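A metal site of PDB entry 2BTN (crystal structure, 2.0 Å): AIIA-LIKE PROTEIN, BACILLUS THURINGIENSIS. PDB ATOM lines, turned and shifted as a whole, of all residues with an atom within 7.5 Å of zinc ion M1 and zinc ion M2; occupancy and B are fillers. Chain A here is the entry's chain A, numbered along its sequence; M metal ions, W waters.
A ring nitrogen (ND1) of His 106 sits at hydrogen-bond distance from the side-chain hydroxyl (OG) of Ser 105 (2.9 Å).
The backbone NH (N) of His 237 lies within hydrogen-bond range of the backbone carbonyl oxygen (O) of Tyr 196 (2.9 Å).
ND1 of His 111 is in hydrogen-bond range of OD2 of Asp 52 (2.9 Å).
A ring nitrogen (ND1) of His 171 is in hydrogen-bond range of the backbone carbonyl oxygen of Ala 208.
ND1 of His 237 is in hydrogen-bond range of O of Pro 36 (2.7 Å).
N of Asp 193 is in hydrogen-bond range of NE2 of His 175.
Four residues have an atom within 4 Å of zinc ion M1: Asp 110, His 111, Asp 193 and His 237.
Within 4 Å of zinc ion M2: His 106, His 108, His 171 and Asp 193.
Zinc ion M1 is bound by the side-chain carboxylate (OD2) of Asp 193, a ring nitrogen (NE2) of His 111, a ring nitrogen (NE2) of His 237, water W3, the side-chain carboxylate (OD1) of Asp 110 and water W2.
Zinc ion M1 has six donor atoms within binding distance.
Zinc ion M2 is bound by water W3 (2.1 Å), a ring nitrogen (NE2) of His 171 (2.3 Å), a ring nitrogen (NE2) of His 106 (2.3 Å), a ring nitrogen (ND1) of His 108 (2.3 Å) and the side-chain carboxylate (OD2) of Asp 193 (2.6 Å).
Slightly farther from zinc ion M2 lies water W1 (2.7 Å).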
ATOM      1  N   CYS A  16     -26.555  18.715 -12.159  1.00  0.00           N
ATOM      2  CA  CYS A  16     -27.226  18.375 -10.919  1.00  0.00           C
ATOM      3  C   CYS A  16     -26.715  19.262  -9.796  1.00  0.00           C
ATOM      4  O   CYS A  16     -25.512  19.324  -9.543  1.00  0.00           O
ATOM      5  CB  CYS A  16     -26.982  16.894 -10.589  1.00  0.00           C
ATOM      6  SG  CYS A  16     -28.156  16.272  -9.378  1.00  0.00           S
ATOM      7  N   LEU A  18     -26.347  20.166  -5.846  1.00  0.00           N
ATOM      8  CA  LEU A  18     -26.170  19.464  -4.563  1.00  0.00           C
ATOM      9  C   LEU A  18     -25.590  20.429  -3.559  1.00  0.00           C
ATOM     10  O   LEU A  18     -24.987  21.435  -3.961  1.00  0.00           O
ATOM     11  CB  LEU A  18     -25.125  18.346  -4.697  1.00  0.00           C
ATOM     12  CG  LEU A  18     -25.216  17.200  -5.680  1.00  0.00           C
ATOM     13  CD1 LEU A  18     -24.234  16.154  -5.248  1.00  0.00           C
ATOM     14  CD2 LEU A  18     -26.606  16.614  -5.673  1.00  0.00           C
ATOM     15  N   LEU A  35     -23.107  20.631 -10.413  1.00  0.00           N
ATOM     16  CA  LEU A  35     -22.163  19.650 -10.958  1.00  0.00           C
ATOM     17  C   LEU A  35     -22.506  19.189 -12.357  1.00  0.00           C
ATOM     18  O   LEU A  35     -23.681  18.974 -12.671  1.00  0.00           O
ATOM     19  CB  LEU A  35     -22.129  18.406 -10.047  1.00  0.00           C
ATOM     20  CG  LEU A  35     -21.841  18.586  -8.554  1.00  0.00           C
ATOM     21  CD1 LEU A  35     -22.002  17.232  -7.835  1.00  0.00           C
ATOM     22  CD2 LEU A  35     -20.467  19.158  -8.340  1.00  0.00           C
ATOM     23  N   PRO A  36     -21.494  18.945 -13.194  1.00  0.00           N
ATOM     24  CA  PRO A  36     -21.750  18.419 -14.532  1.00  0.00           C
ATOM     25  C   PRO A  36     -22.112  16.917 -14.498  1.00  0.00           C
ATOM     26  O   PRO A  36     -21.548  16.149 -13.698  1.00  0.00           O
ATOM     27  CB  PRO A  36     -20.409  18.622 -15.250  1.00  0.00           C
ATOM     28  CG  PRO A  36     -19.371  18.460 -14.127  1.00  0.00           C
ATOM     29  CD  PRO A  36     -20.043  19.090 -12.928  1.00  0.00           C
ATOM     30  N   VAL A  37     -23.039  16.526 -15.352  1.00  0.00           N
ATOM     31  CA  VAL A  37     -23.380  15.116 -15.608  1.00  0.00           C
ATOM     32  C   VAL A  37     -22.797  14.714 -16.962  1.00  0.00           C
ATOM     33  O   VAL A  37     -22.883  15.471 -17.938  1.00  0.00           O
ATOM     34  CB  VAL A  37     -24.913  14.861 -15.533  1.00  0.00           C
ATOM     35  CG1 VAL A  37     -25.265  13.384 -15.852  1.00  0.00           C
ATOM     36  CG2 VAL A  37     -25.471  15.215 -14.119  1.00  0.00           C
ATOM     37  N   TRP A  38     -22.151  13.541 -17.007  1.00  0.00           N
ATOM     38  CA  TRP A  38     -21.456  13.062 -18.193  1.00  0.00           C
ATOM     39  C   TRP A  38     -21.963  11.707 -18.663  1.00  0.00           C
ATOM     40  O   TRP A  38     -22.376  10.875 -17.868  1.00  0.00           O
ATOM     41  CB  TRP A  38     -19.983  12.836 -17.878  1.00  0.00           C
ATOM     42  CG  TRP A  38     -19.201  14.080 -17.574  1.00  0.00           C
ATOM     43  CD1 TRP A  38     -18.738  14.475 -16.339  1.00  0.00           C
ATOM     44  CD2 TRP A  38     -18.771  15.062 -18.505  1.00  0.00           C
ATOM     45  NE1 TRP A  38     -18.039  15.648 -16.455  1.00  0.00           N
ATOM     46  CE2 TRP A  38     -18.034  16.027 -17.774  1.00  0.00           C
ATOM     47  CE3 TRP A  38     -18.908  15.218 -19.897  1.00  0.00           C
ATOM     48  CZ2 TRP A  38     -17.449  17.147 -18.396  1.00  0.00           C
ATOM     49  CZ3 TRP A  38     -18.324  16.320 -20.505  1.00  0.00           C
ATOM     50  CH2 TRP A  38     -17.602  17.271 -19.752  1.00  0.00           C
ATOM     51  N   ASP A  52     -22.673   5.050 -19.351  1.00  0.00           N
ATOM     52  CA  ASP A  52     -23.725   5.810 -18.644  1.00  0.00           C
ATOM     53  C   ASP A  52     -24.782   6.446 -19.557  1.00  0.00           C
ATOM     54  O   ASP A  52     -24.535   6.638 -20.764  1.00  0.00           O
ATOM     55  CB  ASP A  52     -23.135   6.801 -17.634  1.00  0.00           C
ATOM     56  CG  ASP A  52     -22.467   6.101 -16.476  1.00  0.00           C
ATOM     57  OD1 ASP A  52     -22.749   4.887 -16.305  1.00  0.00           O
ATOM     58  OD2 ASP A  52     -21.642   6.655 -15.704  1.00  0.00           O
ATOM     59  N   SER A 105     -21.617   2.513 -14.975  1.00  0.00           N
ATOM     60  CA  SER A 105     -20.619   2.655 -13.913  1.00  0.00           C
ATOM     61  C   SER A 105     -21.278   2.312 -12.583  1.00  0.00           C
ATOM     62  O   SER A 105     -20.675   1.692 -11.719  1.00  0.00           O
ATOM     63  CB  SER A 105     -20.086   4.084 -13.869  1.00  0.00           C
ATOM     64  OG  SER A 105     -21.143   5.007 -13.578  1.00  0.00           O
ATOM     65  N   HIS A 106     -22.549   2.732 -12.445  1.00  0.00           N
ATOM     66  CA  HIS A 106     -23.412   2.378 -11.342  1.00  0.00           C
ATOM     67  C   HIS A 106     -24.856   2.827 -11.660  1.00  0.00           C
ATOM     68  O   HIS A 106     -25.115   3.402 -12.726  1.00  0.00           O
ATOM     69  CB  HIS A 106     -22.890   2.921 -10.004  1.00  0.00           C
ATOM     70  CG  HIS A 106     -22.803   4.421  -9.926  1.00  0.00           C
ATOM     71  ND1 HIS A 106     -22.183   5.193 -10.889  1.00  0.00           N
ATOM     72  CD2 HIS A 106     -23.188   5.278  -8.955  1.00  0.00           C
ATOM     73  CE1 HIS A 106     -22.211   6.460 -10.515  1.00  0.00           C
ATOM     74  NE2 HIS A 106     -22.807   6.535  -9.343  1.00  0.00           N
ATOM     75  N   LEU A 107     -25.799   2.544 -10.759  1.00  0.00           N
ATOM     76  CA  LEU A 107     -27.194   2.768 -11.097  1.00  0.00           C
ATOM     77  C   LEU A 107     -27.831   3.975 -10.382  1.00  0.00           C
ATOM     78  O   LEU A 107     -29.059   4.074 -10.282  1.00  0.00           O
ATOM     79  CB  LEU A 107     -28.019   1.470 -10.964  1.00  0.00           C
ATOM     80  CG  LEU A 107     -27.594   0.268 -11.831  1.00  0.00           C
ATOM     81  CD1 LEU A 107     -28.414  -0.987 -11.457  1.00  0.00           C
ATOM     82  CD2 LEU A 107     -27.678   0.576 -13.359  1.00  0.00           C
ATOM     83  N   HIS A 108     -26.994   4.901  -9.920  1.00  0.00           N
ATOM     84  CA  HIS A 108     -27.518   6.176  -9.392  1.00  0.00           C
ATOM     85  C   HIS A 108     -28.244   6.900 -10.518  1.00  0.00           C
ATOM     86  O   HIS A 108     -27.951   6.660 -11.693  1.00  0.00           O
ATOM     87  CB  HIS A 108     -26.408   7.039  -8.796  1.00  0.00           C
ATOM     88  CG  HIS A 108     -25.937   6.548  -7.457  1.00  0.00           C
ATOM     89  ND1 HIS A 108     -24.865   7.097  -6.793  1.00  0.00           N
ATOM     90  CD2 HIS A 108     -26.415   5.562  -6.660  1.00  0.00           C
ATOM     91  CE1 HIS A 108     -24.703   6.480  -5.646  1.00  0.00           C
ATOM     92  NE2 HIS A 108     -25.623   5.539  -5.540  1.00  0.00           N
ATOM     93  N   PHE A 109     -29.183   7.764 -10.147  1.00  0.00           N
ATOM     94  CA  PHE A 109     -30.134   8.338 -11.114  1.00  0.00           C
ATOM     95  C   PHE A 109     -29.450   9.134 -12.255  1.00  0.00           C
ATOM     96  O   PHE A 109     -30.013   9.237 -13.347  1.00  0.00           O
ATOM     97  CB  PHE A 109     -31.208   9.176 -10.402  1.00  0.00           C
ATOM     98  CG  PHE A 109     -30.783  10.579 -10.128  1.00  0.00           C
ATOM     99  CD1 PHE A 109     -31.155  11.621 -10.991  1.00  0.00           C
ATOM    100  CD2 PHE A 109     -29.964  10.874  -9.042  1.00  0.00           C
ATOM    101  CE1 PHE A 109     -30.747  12.932 -10.762  1.00  0.00           C
ATOM    102  CE2 PHE A 109     -29.530  12.166  -8.812  1.00  0.00           C
ATOM    103  CZ  PHE A 109     -29.922  13.198  -9.667  1.00  0.00           C
ATOM    104  N   ASP A 110     -28.272   9.697 -11.997  1.00  0.00           N
ATOM    105  CA  ASP A 110     -27.580  10.530 -12.980  1.00  0.00           C
ATOM    106  C   ASP A 110     -26.636   9.742 -13.915  1.00  0.00           C
ATOM    107  O   ASP A 110     -25.961  10.343 -14.777  1.00  0.00           O
ATOM    108  CB  ASP A 110     -26.840  11.708 -12.293  1.00  0.00           C
ATOM    109  CG  ASP A 110     -25.963  11.244 -11.134  1.00  0.00           C
ATOM    110  OD1 ASP A 110     -24.806  11.719 -11.036  1.00  0.00           O
ATOM    111  OD2 ASP A 110     -26.325  10.398 -10.304  1.00  0.00           O
ATOM    112  N   HIS A 111     -26.606   8.419 -13.751  1.00  0.00           N
ATOM    113  CA  HIS A 111     -25.765   7.517 -14.552  1.00  0.00           C
ATOM    114  C   HIS A 111     -26.572   6.449 -15.295  1.00  0.00           C
ATOM    115  O   HIS A 111     -26.109   5.978 -16.313  1.00  0.00           O
ATOM    116  CB  HIS A 111     -24.700   6.865 -13.652  1.00  0.00           C
ATOM    117  CG  HIS A 111     -23.832   7.868 -12.974  1.00  0.00           C
ATOM    118  ND1 HIS A 111     -22.614   8.260 -13.483  1.00  0.00           N
ATOM    119  CD2 HIS A 111     -24.048   8.647 -11.896  1.00  0.00           C
ATOM    120  CE1 HIS A 111     -22.108   9.203 -12.724  1.00  0.00           C
ATOM    121  NE2 HIS A 111     -22.956   9.457 -11.745  1.00  0.00           N
ATOM    122  N   GLU A 129     -23.927  -3.990  -7.593  1.00  0.00           N
ATOM    123  CA  GLU A 129     -24.711  -2.787  -7.905  1.00  0.00           C
ATOM    124  C   GLU A 129     -26.145  -3.165  -8.273  1.00  0.00           C
ATOM    125  O   GLU A 129     -27.112  -2.600  -7.745  1.00  0.00           O
ATOM    126  CB  GLU A 129     -24.098  -1.969  -9.049  1.00  0.00           C
ATOM    127  CG  GLU A 129     -24.761  -0.600  -9.309  1.00  0.00           C
ATOM    128  CD  GLU A 129     -24.539   0.389  -8.187  1.00  0.00           C
ATOM    129  OE1 GLU A 129     -23.650   0.143  -7.349  1.00  0.00           O
ATOM    130  OE2 GLU A 129     -25.277   1.409  -8.128  1.00  0.00           O
ATOM    131  N   HIS A 171     -18.481   4.308  -3.258  1.00  0.00           N
ATOM    132  CA  HIS A 171     -19.427   5.368  -3.576  1.00  0.00           C
ATOM    133  C   HIS A 171     -20.837   4.771  -3.722  1.00  0.00           C
ATOM    134  O   HIS A 171     -21.817   5.356  -3.259  1.00  0.00           O
ATOM    135  CB  HIS A 171     -19.053   6.131  -4.843  1.00  0.00           C
ATOM    136  CG  HIS A 171     -20.112   7.086  -5.283  1.00  0.00           C
ATOM    137  ND1 HIS A 171     -20.358   8.270  -4.613  1.00  0.00           N
ATOM    138  CD2 HIS A 171     -21.049   6.998  -6.248  1.00  0.00           C
ATOM    139  CE1 HIS A 171     -21.370   8.892  -5.181  1.00  0.00           C
ATOM    140  NE2 HIS A 171     -21.820   8.135  -6.164  1.00  0.00           N
ATOM    141  N   SER A 172     -20.930   3.621  -4.379  1.00  0.00           N
ATOM    142  CA  SER A 172     -22.147   2.810  -4.381  1.00  0.00           C
ATOM    143  C   SER A 172     -21.688   1.365  -4.177  1.00  0.00           C
ATOM    144  O   SER A 172     -20.488   1.054  -4.358  1.00  0.00           O
ATOM    145  CB  SER A 172     -22.913   3.001  -5.699  1.00  0.00           C
ATOM    146  OG  SER A 172     -22.194   2.463  -6.804  1.00  0.00           O
ATOM    147  N   HIS A 175     -19.948   0.155  -7.604  1.00  0.00           N
ATOM    148  CA  HIS A 175     -19.449   1.174  -8.512  1.00  0.00           C
ATOM    149  C   HIS A 175     -18.250   0.666  -9.317  1.00  0.00           C
ATOM    150  O   HIS A 175     -17.384  -0.008  -8.773  1.00  0.00           O
ATOM    151  CB  HIS A 175     -19.066   2.447  -7.746  1.00  0.00           C
ATOM    152  CG  HIS A 175     -18.628   3.554  -8.657  1.00  0.00           C
ATOM    153  ND1 HIS A 175     -17.342   3.653  -9.138  1.00  0.00           N
ATOM    154  CD2 HIS A 175     -19.323   4.562  -9.223  1.00  0.00           C
ATOM    155  CE1 HIS A 175     -17.255   4.697  -9.940  1.00  0.00           C
ATOM    156  NE2 HIS A 175     -18.447   5.268 -10.012  1.00  0.00           N
ATOM    157  N   ILE A 192     -15.192   8.078 -12.888  1.00  0.00           N
ATOM    158  CA  ILE A 192     -16.611   8.270 -12.620  1.00  0.00           C
ATOM    159  C   ILE A 192     -16.740   8.708 -11.144  1.00  0.00           C
ATOM    160  O   ILE A 192     -15.993   9.581 -10.730  1.00  0.00           O
ATOM    161  CB  ILE A 192     -17.504   7.009 -12.962  1.00  0.00           C
ATOM    162  CG1 ILE A 192     -16.988   6.283 -14.215  1.00  0.00           C
ATOM    163  CG2 ILE A 192     -19.002   7.414 -13.061  1.00  0.00           C
ATOM    164  CD1 ILE A 192     -17.072   7.074 -15.538  1.00  0.00           C
ATOM    165  N   ASP A 193     -17.682   8.137 -10.378  1.00  0.00           N
ATOM    166  CA  ASP A 193     -17.928   8.605  -9.023  1.00  0.00           C
ATOM    167  C   ASP A 193     -17.045   7.988  -7.926  1.00  0.00           C
ATOM    168  O   ASP A 193     -17.261   8.238  -6.758  1.00  0.00           O
ATOM    169  CB  ASP A 193     -19.412   8.502  -8.651  1.00  0.00           C
ATOM    170  CG  ASP A 193     -20.272   9.506  -9.412  1.00  0.00           C
ATOM    171  OD1 ASP A 193     -19.773  10.137 -10.395  1.00  0.00           O
ATOM    172  OD2 ASP A 193     -21.449   9.740  -9.076  1.00  0.00           O
ATOM    173  N   ALA A 194     -16.032   7.210  -8.322  1.00  0.00           N
ATOM    174  CA  ALA A 194     -14.972   6.822  -7.405  1.00  0.00           C
ATOM    175  C   ALA A 194     -14.193   8.054  -6.882  1.00  0.00           C
ATOM    176  O   ALA A 194     -13.549   7.978  -5.847  1.00  0.00           O
ATOM    177  CB  ALA A 194     -14.046   5.819  -8.058  1.00  0.00           C
ATOM    178  N   TYR A 196     -15.274  12.418  -7.266  1.00  0.00           N
ATOM    179  CA  TYR A 196     -15.989  13.528  -7.932  1.00  0.00           C
ATOM    180  C   TYR A 196     -15.013  14.548  -8.506  1.00  0.00           C
ATOM    181  O   TYR A 196     -15.181  15.035  -9.619  1.00  0.00           O
ATOM    182  CB  TYR A 196     -16.891  14.266  -6.923  1.00  0.00           C
ATOM    183  CG  TYR A 196     -18.230  13.667  -6.522  1.00  0.00           C
ATOM    184  CD1 TYR A 196     -18.590  12.354  -6.824  1.00  0.00           C
ATOM    185  CD2 TYR A 196     -19.143  14.443  -5.789  1.00  0.00           C
ATOM    186  CE1 TYR A 196     -19.847  11.819  -6.433  1.00  0.00           C
ATOM    187  CE2 TYR A 196     -20.382  13.929  -5.389  1.00  0.00           C
ATOM    188  CZ  TYR A 196     -20.726  12.636  -5.706  1.00  0.00           C
ATOM    189  OH  TYR A 196     -21.944  12.180  -5.285  1.00  0.00           O
ATOM    190  N   ALA A 208     -19.482  12.170  -0.627  1.00  0.00           N
ATOM    191  CA  ALA A 208     -20.706  11.381  -0.446  1.00  0.00           C
ATOM    192  C   ALA A 208     -20.542   9.953  -0.961  1.00  0.00           C
ATOM    193  O   ALA A 208     -19.910   9.715  -2.002  1.00  0.00           O
ATOM    194  CB  ALA A 208     -21.897  12.062  -1.119  1.00  0.00           C
ATOM    195  N   GLY A 236     -15.392  12.426 -11.872  1.00  0.00           N
ATOM    196  CA  GLY A 236     -16.804  12.235 -12.179  1.00  0.00           C
ATOM    197  C   GLY A 236     -17.645  13.498 -12.250  1.00  0.00           C
ATOM    198  O   GLY A 236     -18.521  13.605 -13.085  1.00  0.00           O
ATOM    199  N   HIS A 237     -17.392  14.452 -11.362  1.00  0.00           N
ATOM    200  CA  HIS A 237     -18.261  15.628 -11.245  1.00  0.00           C
ATOM    201  C   HIS A 237     -17.411  16.850 -10.901  1.00  0.00           C
ATOM    202  O   HIS A 237     -17.567  17.453  -9.842  1.00  0.00           O
ATOM    203  CB  HIS A 237     -19.318  15.388 -10.165  1.00  0.00           C
ATOM    204  CG  HIS A 237     -20.338  14.356 -10.524  1.00  0.00           C
ATOM    205  ND1 HIS A 237     -21.224  14.513 -11.557  1.00  0.00           N
ATOM    206  CD2 HIS A 237     -20.670  13.180  -9.936  1.00  0.00           C
ATOM    207  CE1 HIS A 237     -22.026  13.466 -11.633  1.00  0.00           C
ATOM    208  NE2 HIS A 237     -21.707  12.644 -10.646  1.00  0.00           N
HETATM  209 ZN    ZN M   1     -22.861  10.858 -10.132  1.00  0.00          ZN
HETATM  210 ZN    ZN M   2     -23.233   8.256  -7.927  1.00  0.00          ZN
HETATM  211  O   HOH W   1     -23.277  10.466  -6.422  1.00  0.00           O
HETATM  212  O   HOH W   2     -23.655  11.986  -7.983  1.00  0.00           O
HETATM  213  O   HOH W   3     -24.303   9.790  -8.816  1.00  0.00           O
